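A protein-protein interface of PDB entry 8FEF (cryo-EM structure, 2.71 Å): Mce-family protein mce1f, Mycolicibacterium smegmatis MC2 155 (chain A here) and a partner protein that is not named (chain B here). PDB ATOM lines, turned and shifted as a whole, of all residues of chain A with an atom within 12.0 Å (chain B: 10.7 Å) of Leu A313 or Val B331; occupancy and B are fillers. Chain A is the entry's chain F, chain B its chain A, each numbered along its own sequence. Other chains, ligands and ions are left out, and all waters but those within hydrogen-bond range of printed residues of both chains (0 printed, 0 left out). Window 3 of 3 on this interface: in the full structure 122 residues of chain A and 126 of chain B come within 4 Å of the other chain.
N of Leu A309 is in hydrogen-bond range of O of Asn B327, at 2.9 Å. The side-chain hydroxyl (OG) of Ser B328 sits at hydrogen-bond distance from the backbone carbonyl oxygen (O) of Leu A309, at 3.2 Å. N of Phe A311 lies within hydrogen-bond range of O of Leu B329, 3.3 Å away. The backbone carbonyl oxygen (O) of Phe A311 lies within hydrogen-bond range of the backbone NH (N) of Val B331 (2.8 Å). N of Leu A313 is in hydrogen-bond range of O of Val B331.
CB of Asn B327 touches CD2 of Leu A308 (3.7 Å). O of Leu B329 touches CB of His A310, 3.3 Å away. Ser B328 touches Phe A311. Phe A311 touches Val B330. CA of Gly A312 touches O of Val B331, at 3.2 Å. Val B333 touches Gly A312. O of Leu A313 touches CG2 of Val B333, at 3.8 Å.
Of the printed residues of chain B, Leu A308 touches Asn B327 (3.7 Å). Printed residues of chain B within 4 Å of His A310: Leu B329 (3.3 Å). Printed residues of chain B within 4 Å of Phe A311: Ser B328, Leu B329, Val B330 and Val B331. Leu A313 touches just these residues of chain B: Val B331 and Val B333. Leu B329 touches just these residues of chain A: His A310 (3.3 Å) and Phe A311 (3.3 Å). Of chain A, only Phe A311 comes within 4 Å of Val B330. No residue of chain A comes within 4 Å of Gly B332. Of chain A, only Gly A312 and Leu A313 come within 4 Å of Val B333. The nearest residue of chain B that does not touch Leu A313 is Val B330 (4.1 Å). The nearest residue of chain A that does not touch Val B331 is His A310 (4.1 Å). The nearest printed residue of chain B that does not touch Phe A311 is Gly B332 (5.3 Å).
Printed residues of chain A that touch a printed residue of chain B: Leu A308, Leu A309, His A310, Phe A311, Gly A312 and Leu A313. Of the 19 printed residues of chain B, 6 touch a printed residue of chain A. Printed residues of chain B that touch a printed residue of chain A: Asn B327, Ser B328, Leu B329, Val B330, Val B331 and Val B333. Among the printed residues, 12 pairs touch across the chains.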
ATOM      1  N   LEU A 308      24.055  21.109  17.720  1.00  0.00           N
ATOM      2  CA  LEU A 308      23.723  20.018  16.813  1.00  0.00           C
ATOM      3  C   LEU A 308      22.219  19.952  16.576  1.00  0.00           C
ATOM      4  O   LEU A 308      21.426  19.980  17.522  1.00  0.00           O
ATOM      5  CB  LEU A 308      24.231  18.694  17.379  1.00  0.00           C
ATOM      6  CG  LEU A 308      25.748  18.587  17.526  1.00  0.00           C
ATOM      7  CD1 LEU A 308      26.134  17.315  18.254  1.00  0.00           C
ATOM      8  CD2 LEU A 308      26.405  18.641  16.161  1.00  0.00           C
ATOM      9  N   LEU A 309      21.830  19.862  15.304  1.00  0.00           N
ATOM     10  CA  LEU A 309      20.420  19.778  14.924  1.00  0.00           C
ATOM     11  C   LEU A 309      20.369  19.035  13.595  1.00  0.00           C
ATOM     12  O   LEU A 309      20.648  19.619  12.545  1.00  0.00           O
ATOM     13  CB  LEU A 309      19.792  21.163  14.826  1.00  0.00           C
ATOM     14  CG  LEU A 309      18.265  21.285  14.830  1.00  0.00           C
ATOM     15  CD1 LEU A 309      17.862  22.655  15.339  1.00  0.00           C
ATOM     16  CD2 LEU A 309      17.666  21.045  13.456  1.00  0.00           C
ATOM     17  N   HIS A 310      20.001  17.760  13.648  1.00  0.00           N
ATOM     18  CA  HIS A 310      20.008  16.895  12.480  1.00  0.00           C
ATOM     19  C   HIS A 310      18.672  16.951  11.748  1.00  0.00           C
ATOM     20  O   HIS A 310      17.660  17.411  12.281  1.00  0.00           O
ATOM     21  CB  HIS A 310      20.317  15.458  12.896  1.00  0.00           C
ATOM     22  CG  HIS A 310      21.417  15.349  13.905  1.00  0.00           C
ATOM     23  ND1 HIS A 310      22.523  16.171  13.892  1.00  0.00           N
ATOM     24  CD2 HIS A 310      21.575  14.524  14.966  1.00  0.00           C
ATOM     25  CE1 HIS A 310      23.319  15.851  14.896  1.00  0.00           C
ATOM     26  NE2 HIS A 310      22.766  14.855  15.565  1.00  0.00           N
ATOM     27  N   PHE A 311      18.682  16.475  10.507  1.00  0.00           N
ATOM     28  CA  PHE A 311      17.493  16.423   9.669  1.00  0.00           C
ATOM     29  C   PHE A 311      17.226  14.981   9.277  1.00  0.00           C
ATOM     30  O   PHE A 311      18.137  14.275   8.834  1.00  0.00           O
ATOM     31  CB  PHE A 311      17.654  17.286   8.417  1.00  0.00           C
ATOM     32  CG  PHE A 311      17.697  18.756   8.696  1.00  0.00           C
ATOM     33  CD1 PHE A 311      16.983  19.292   9.753  1.00  0.00           C
ATOM     34  CD2 PHE A 311      18.450  19.603   7.904  1.00  0.00           C
ATOM     35  CE1 PHE A 311      17.018  20.645  10.012  1.00  0.00           C
ATOM     36  CE2 PHE A 311      18.490  20.956   8.160  1.00  0.00           C
ATOM     37  CZ  PHE A 311      17.773  21.478   9.216  1.00  0.00           C
ATOM     38  N   GLY A 312      15.981  14.543   9.442  1.00  0.00           N
ATOM     39  CA  GLY A 312      15.608  13.183   9.118  1.00  0.00           C
ATOM     40  C   GLY A 312      15.168  13.013   7.679  1.00  0.00           C
ATOM     41  O   GLY A 312      14.360  13.795   7.170  1.00  0.00           O
ATOM     42  N   LEU A 313      15.702  11.986   7.027  1.00  0.00           N
ATOM     43  CA  LEU A 313      15.338  11.691   5.652  1.00  0.00           C
ATOM     44  C   LEU A 313      13.958  11.042   5.592  1.00  0.00           C
ATOM     45  O   LEU A 313      13.480  10.439   6.556  1.00  0.00           O
ATOM     46  CB  LEU A 313      16.379  10.778   5.005  1.00  0.00           C
ATOM     47  CG  LEU A 313      17.740  11.407   4.710  1.00  0.00           C
ATOM     48  CD1 LEU A 313      18.702  10.368   4.159  1.00  0.00           C
ATOM     49  CD2 LEU A 313      17.588  12.568   3.741  1.00  0.00           C
ATOM     50  N   GLY A 314      13.319  11.170   4.433  1.00  0.00           N
ATOM     51  CA  GLY A 314      11.979  10.650   4.242  1.00  0.00           C
ATOM     52  C   GLY A 314      10.934  11.740   4.160  1.00  0.00           C
ATOM     53  O   GLY A 314      10.910  12.647   4.998  1.00  0.00           O
ATOM     54  N   ILE A 315      10.056  11.661   3.164  1.00  0.00           N
ATOM     55  CA  ILE A 315       9.084  12.710   2.880  1.00  0.00           C
ATOM     56  C   ILE A 315       7.706  12.238   3.321  1.00  0.00           C
ATOM     57  O   ILE A 315       7.270  11.142   2.950  1.00  0.00           O
ATOM     58  CB  ILE A 315       9.095  13.101   1.392  1.00  0.00           C
ATOM     59  CG1 ILE A 315       9.006  11.865   0.495  1.00  0.00           C
ATOM     60  CG2 ILE A 315      10.346  13.901   1.063  1.00  0.00           C
ATOM     61  CD1 ILE A 315       8.900  12.186  -0.976  1.00  0.00           C
ATOM     62  N   ASN A 316       7.034  13.062   4.130  1.00  0.00           N
ATOM     63  CA  ASN A 316       5.660  12.815   4.576  1.00  0.00           C
ATOM     64  C   ASN A 316       5.522  11.463   5.275  1.00  0.00           C
ATOM     65  O   ASN A 316       4.592  10.699   5.011  1.00  0.00           O
ATOM     66  CB  ASN A 316       4.681  12.915   3.403  1.00  0.00           C
ATOM     67  CG  ASN A 316       4.259  14.335   3.113  1.00  0.00           C
ATOM     68  OD1 ASN A 316       4.875  15.289   3.584  1.00  0.00           O
ATOM     69  ND2 ASN A 316       3.201  14.486   2.326  1.00  0.00           N
ATOM     70  N   ALA A 317       6.468  11.157   6.166  1.00  0.00           N
ATOM     71  CA  ALA A 317       6.336   9.909   6.908  1.00  0.00           C
ATOM     72  C   ALA A 317       5.140  10.022   7.863  1.00  0.00           C
ATOM     73  O   ALA A 317       4.172   9.278   7.665  1.00  0.00           O
ATOM     74  CB  ALA A 317       7.661   9.514   7.578  1.00  0.00           C
ATOM     75  N   PRO A 318       5.115  10.888   8.886  1.00  0.00           N
ATOM     76  CA  PRO A 318       3.823  11.409   9.334  1.00  0.00           C
ATOM     77  C   PRO A 318       3.530  12.752   8.693  1.00  0.00           C
ATOM     78  O   PRO A 318       4.353  13.678   8.764  1.00  0.00           O
ATOM     79  CB  PRO A 318       3.993  11.533  10.854  1.00  0.00           C
ATOM     80  CG  PRO A 318       5.445  11.631  11.083  1.00  0.00           C
ATOM     81  CD  PRO A 318       6.173  11.371   9.797  1.00  0.00           C
ATOM     82  N   PRO A 319       2.370  12.909   8.056  1.00  0.00           N
ATOM     83  CA  PRO A 319       2.013  14.216   7.518  1.00  0.00           C
ATOM     84  C   PRO A 319       1.657  15.176   8.637  1.00  0.00           C
ATOM     85  O   PRO A 319       1.212  14.754   9.718  1.00  0.00           O
ATOM     86  CB  PRO A 319       0.795  13.911   6.628  1.00  0.00           C
ATOM     87  CG  PRO A 319       0.203  12.693   7.229  1.00  0.00           C
ATOM     88  CD  PRO A 319       1.357  11.885   7.754  1.00  0.00           C
ATOM     89  N   ASN B 327      24.492  22.805  13.457  1.00  0.00           N
ATOM     90  CA  ASN B 327      25.211  21.825  12.651  1.00  0.00           C
ATOM     91  C   ASN B 327      24.227  20.750  12.207  1.00  0.00           C
ATOM     92  O   ASN B 327      23.654  20.045  13.045  1.00  0.00           O
ATOM     93  CB  ASN B 327      26.361  21.204  13.441  1.00  0.00           C
ATOM     94  CG  ASN B 327      27.708  21.442  12.794  1.00  0.00           C
ATOM     95  OD1 ASN B 327      27.798  21.677  11.590  1.00  0.00           O
ATOM     96  ND2 ASN B 327      28.768  21.373  13.590  1.00  0.00           N
ATOM     97  N   SER B 328      24.041  20.616  10.898  1.00  0.00           N
ATOM     98  CA  SER B 328      23.014  19.749  10.340  1.00  0.00           C
ATOM     99  C   SER B 328      23.654  18.604   9.569  1.00  0.00           C
ATOM    100  O   SER B 328      24.484  18.831   8.686  1.00  0.00           O
ATOM    101  CB  SER B 328      22.073  20.537   9.429  1.00  0.00           C
ATOM    102  OG  SER B 328      21.411  21.558  10.152  1.00  0.00           O
ATOM    103  N   LEU B 329      23.268  17.379   9.912  1.00  0.00           N
ATOM    104  CA  LEU B 329      23.640  16.189   9.162  1.00  0.00           C
ATOM    105  C   LEU B 329      22.408  15.316   8.987  1.00  0.00           C
ATOM    106  O   LEU B 329      21.617  15.156   9.921  1.00  0.00           O
ATOM    107  CB  LEU B 329      24.762  15.417   9.872  1.00  0.00           C
ATOM    108  CG  LEU B 329      24.595  15.124  11.367  1.00  0.00           C
ATOM    109  CD1 LEU B 329      23.995  13.749  11.611  1.00  0.00           C
ATOM    110  CD2 LEU B 329      25.918  15.268  12.099  1.00  0.00           C
ATOM    111  N   VAL B 330      22.234  14.768   7.782  1.00  0.00           N
ATOM    112  CA  VAL B 330      21.061  13.947   7.511  1.00  0.00           C
ATOM    113  C   VAL B 330      21.156  12.638   8.287  1.00  0.00           C
ATOM    114  O   VAL B 330      22.244  12.092   8.506  1.00  0.00           O
ATOM    115  CB  VAL B 330      20.903  13.698   6.000  1.00  0.00           C
ATOM    116  CG1 VAL B 330      20.641  15.009   5.275  1.00  0.00           C
ATOM    117  CG2 VAL B 330      22.137  13.020   5.434  1.00  0.00           C
ATOM    118  N   VAL B 331      20.002  12.136   8.725  1.00  0.00           N
ATOM    119  CA  VAL B 331      19.924  10.959   9.582  1.00  0.00           C
ATOM    120  C   VAL B 331      18.599  10.255   9.303  1.00  0.00           C
ATOM    121  O   VAL B 331      17.722  10.787   8.618  1.00  0.00           O
ATOM    122  CB  VAL B 331      20.053  11.340  11.077  1.00  0.00           C
ATOM    123  CG1 VAL B 331      18.735  11.884  11.609  1.00  0.00           C
ATOM    124  CG2 VAL B 331      20.563  10.173  11.917  1.00  0.00           C
ATOM    125  N   GLY B 332      18.459   9.036   9.818  1.00  0.00           N
ATOM    126  CA  GLY B 332      17.207   8.305   9.719  1.00  0.00           C
ATOM    127  C   GLY B 332      16.326   8.524  10.939  1.00  0.00           C
ATOM    128  O   GLY B 332      16.814   8.648  12.061  1.00  0.00           O
ATOM    129  N   VAL B 333      15.018   8.566  10.703  1.00  0.00           N
ATOM    130  CA  VAL B 333      14.029   8.825  11.745  1.00  0.00           C
ATOM    131  C   VAL B 333      13.403   7.515  12.191  1.00  0.00           C
ATOM    132  O   VAL B 333      13.213   6.592  11.389  1.00  0.00           O
ATOM    133  CB  VAL B 333      12.948   9.819  11.280  1.00  0.00           C
ATOM    134  CG1 VAL B 333      13.556  11.154  11.015  1.00  0.00           C
ATOM    135  CG2 VAL B 333      12.285   9.320  10.021  1.00  0.00           C
ATOM    136  N   GLY B 334      13.088   7.432  13.475  1.00  0.00           N
ATOM    137  CA  GLY B 334      12.446   6.255  14.011  1.00  0.00           C
ATOM    138  C   GLY B 334      11.007   6.129  13.552  1.00  0.00           C
ATOM    139  O   GLY B 334      10.425   7.021  12.933  1.00  0.00           O
ATOM    140  N   ASN B 335      10.429   4.974  13.859  1.00  0.00           N
ATOM    141  CA  ASN B 335       9.065   4.691  13.447  1.00  0.00           C
ATOM    142  C   ASN B 335       8.090   5.596  14.197  1.00  0.00           C
ATOM    143  O   ASN B 335       8.312   5.908  15.371  1.00  0.00           O
ATOM    144  CB  ASN B 335       8.728   3.226  13.710  1.00  0.00           C
ATOM    145  CG  ASN B 335       9.679   2.281  13.013  1.00  0.00           C
ATOM    146  OD1 ASN B 335      10.162   2.565  11.918  1.00  0.00           O
ATOM    147  ND2 ASN B 335       9.960   1.150  13.648  1.00  0.00           N
ATOM    148  N   PRO B 336       7.015   6.041  13.544  1.00  0.00           N
ATOM    149  CA  PRO B 336       6.057   6.929  14.211  1.00  0.00           C
ATOM    150  C   PRO B 336       5.405   6.257  15.408  1.00  0.00           C
ATOM    151  O   PRO B 336       5.352   5.030  15.520  1.00  0.00           O
ATOM    152  CB  PRO B 336       5.025   7.229  13.116  1.00  0.00           C
ATOM    153  CG  PRO B 336       5.729   6.945  11.838  1.00  0.00           C
ATOM    154  CD  PRO B 336       6.674   5.824  12.130  1.00  0.00           C
ATOM    155  N   TRP B 367      31.081  11.846  25.961  1.00  0.00           N
ATOM    156  CA  TRP B 367      30.166  12.689  25.202  1.00  0.00           C
ATOM    157  C   TRP B 367      28.710  12.225  25.231  1.00  0.00           C
ATOM    158  O   TRP B 367      27.841  13.022  25.601  1.00  0.00           O
ATOM    159  CB  TRP B 367      30.627  12.827  23.753  1.00  0.00           C
ATOM    160  CG  TRP B 367      29.595  13.468  22.897  1.00  0.00           C
ATOM    161  CD1 TRP B 367      29.053  14.704  23.062  1.00  0.00           C
ATOM    162  CD2 TRP B 367      28.966  12.903  21.743  1.00  0.00           C
ATOM    163  NE1 TRP B 367      28.130  14.950  22.078  1.00  0.00           N
ATOM    164  CE2 TRP B 367      28.057  13.859  21.256  1.00  0.00           C
ATOM    165  CE3 TRP B 367      29.087  11.684  21.072  1.00  0.00           C
ATOM    166  CZ2 TRP B 367      27.276  13.636  20.131  1.00  0.00           C
ATOM    167  CZ3 TRP B 367      28.310  11.466  19.957  1.00  0.00           C
ATOM    168  CH2 TRP B 367      27.416  12.436  19.497  1.00  0.00           C
ATOM    169  N   TYR B 383      16.379   1.420  19.228  1.00  0.00           N
ATOM    170  CA  TYR B 383      17.012   1.803  17.967  1.00  0.00           C
ATOM    171  C   TYR B 383      18.527   1.613  18.050  1.00  0.00           C
ATOM    172  O   TYR B 383      19.311   2.558  17.979  1.00  0.00           O
ATOM    173  CB  TYR B 383      16.650   3.240  17.609  1.00  0.00           C
ATOM    174  CG  TYR B 383      15.212   3.419  17.187  1.00  0.00           C
ATOM    175  CD1 TYR B 383      14.792   3.056  15.918  1.00  0.00           C
ATOM    176  CD2 TYR B 383      14.276   3.959  18.057  1.00  0.00           C
ATOM    177  CE1 TYR B 383      13.480   3.220  15.528  1.00  0.00           C
ATOM    178  CE2 TYR B 383      12.962   4.127  17.675  1.00  0.00           C
ATOM    179  CZ  TYR B 383      12.570   3.755  16.410  1.00  0.00           C
ATOM    180  OH  TYR B 383      11.263   3.919  16.021  1.00  0.00           O
ATOM    181  N   HIS B 385      20.198  -0.432  15.914  1.00  0.00           N
ATOM    182  CA  HIS B 385      20.674  -1.021  14.673  1.00  0.00           C
ATOM    183  C   HIS B 385      19.980  -0.347  13.496  1.00  0.00           C
ATOM    184  O   HIS B 385      18.995   0.378  13.658  1.00  0.00           O
ATOM    185  CB  HIS B 385      20.513  -2.545  14.721  1.00  0.00           C
ATOM    186  CG  HIS B 385      19.104  -3.005  14.918  1.00  0.00           C
ATOM    187  ND1 HIS B 385      18.460  -2.922  16.134  1.00  0.00           N
ATOM    188  CD2 HIS B 385      18.243  -3.623  14.081  1.00  0.00           C
ATOM    189  CE1 HIS B 385      17.242  -3.420  16.021  1.00  0.00           C
ATOM    190  NE2 HIS B 385      17.086  -3.852  14.784  1.00  0.00           N
ATOM    191  N   PHE B 386      20.509  -0.598  12.301  1.00  0.00           N
ATOM    192  CA  PHE B 386      19.919  -0.110  11.058  1.00  0.00           C
ATOM    193  C   PHE B 386      18.819  -1.035  10.552  1.00  0.00           C
ATOM    194  O   PHE B 386      19.076  -2.200  10.231  1.00  0.00           O
ATOM    195  CB  PHE B 386      21.011   0.047   9.999  1.00  0.00           C
ATOM    196  CG  PHE B 386      20.489   0.341   8.617  1.00  0.00           C
ATOM    197  CD1 PHE B 386      20.252   1.645   8.225  1.00  0.00           C
ATOM    198  CD2 PHE B 386      20.259  -0.678   7.706  1.00  0.00           C
ATOM    199  CE1 PHE B 386      19.784   1.926   6.959  1.00  0.00           C
ATOM    200  CE2 PHE B 386      19.783  -0.402   6.441  1.00  0.00           C
ATOM    201  CZ  PHE B 386      19.546   0.901   6.067  1.00  0.00           C
ATOM    202  N   GLU B 387      17.593  -0.515  10.484  1.00  0.00           N
ATOM    203  CA  GLU B 387      16.459  -1.254   9.943  1.00  0.00           C
ATOM    204  C   GLU B 387      15.613  -0.358   9.060  1.00  0.00           C
ATOM    205  O   GLU B 387      15.568   0.862   9.237  1.00  0.00           O
ATOM    206  CB  GLU B 387      15.558  -1.845  11.022  1.00  0.00           C
ATOM    207  CG  GLU B 387      16.153  -3.022  11.706  1.00  0.00           C
ATOM    208  CD  GLU B 387      15.113  -3.952  12.269  1.00  0.00           C
ATOM    209  OE1 GLU B 387      13.928  -3.817  11.904  1.00  0.00           O
ATOM    210  OE2 GLU B 387      15.481  -4.813  13.090  1.00  0.00           O
ATOM    211  N   LEU B 388      14.946  -0.988   8.101  1.00  0.00           N
ATOM    212  CA  LEU B 388      14.034  -0.282   7.220  1.00  0.00           C
ATOM    213  C   LEU B 388      12.816   0.179   8.008  1.00  0.00           C
ATOM    214  O   LEU B 388      12.386  -0.472   8.963  1.00  0.00           O
ATOM    215  CB  LEU B 388      13.608  -1.188   6.068  1.00  0.00           C
ATOM    216  CG  LEU B 388      14.724  -2.028   5.441  1.00  0.00           C
ATOM    217  CD1 LEU B 388      14.152  -3.023   4.447  1.00  0.00           C
ATOM    218  CD2 LEU B 388      15.754  -1.133   4.773  1.00  0.00           C
ATOM    219  N   GLY B 389      12.275   1.330   7.618  1.00  0.00           N
ATOM    220  CA  GLY B 389      11.075   1.838   8.251  1.00  0.00           C
ATOM    221  C   GLY B 389       9.910   0.888   8.094  1.00  0.00           C
ATOM    222  O   GLY B 389       9.592   0.476   6.975  1.00  0.00           O
ATOM    223  N   PRO B 391       6.489   1.212   8.509  1.00  0.00           N
ATOM    224  CA  PRO B 391       5.582   1.710   7.454  1.00  0.00           C
ATOM    225  C   PRO B 391       6.375   2.369   6.332  1.00  0.00           C
ATOM    226  O   PRO B 391       6.412   3.595   6.180  1.00  0.00           O
ATOM    227  CB  PRO B 391       4.690   2.699   8.218  1.00  0.00           C
ATOM    228  CG  PRO B 391       5.003   2.512   9.675  1.00  0.00           C
ATOM    229  CD  PRO B 391       6.413   2.063   9.706  1.00  0.00           C
ATOM    230  N   MET B 392       7.048   1.529   5.539  1.00  0.00           N
ATOM    231  CA  MET B 392       7.999   2.020   4.544  1.00  0.00           C
ATOM    232  C   MET B 392       7.321   2.905   3.505  1.00  0.00           C
ATOM    233  O   MET B 392       7.826   3.978   3.167  1.00  0.00           O
ATOM    234  CB  MET B 392       8.695   0.841   3.865  1.00  0.00           C
ATOM    235  CG  MET B 392       9.976   1.211   3.137  1.00  0.00           C
ATOM    236  SD  MET B 392      10.773  -0.214   2.377  1.00  0.00           S
ATOM    237  CE  MET B 392      10.794  -1.362   3.749  1.00  0.00           C
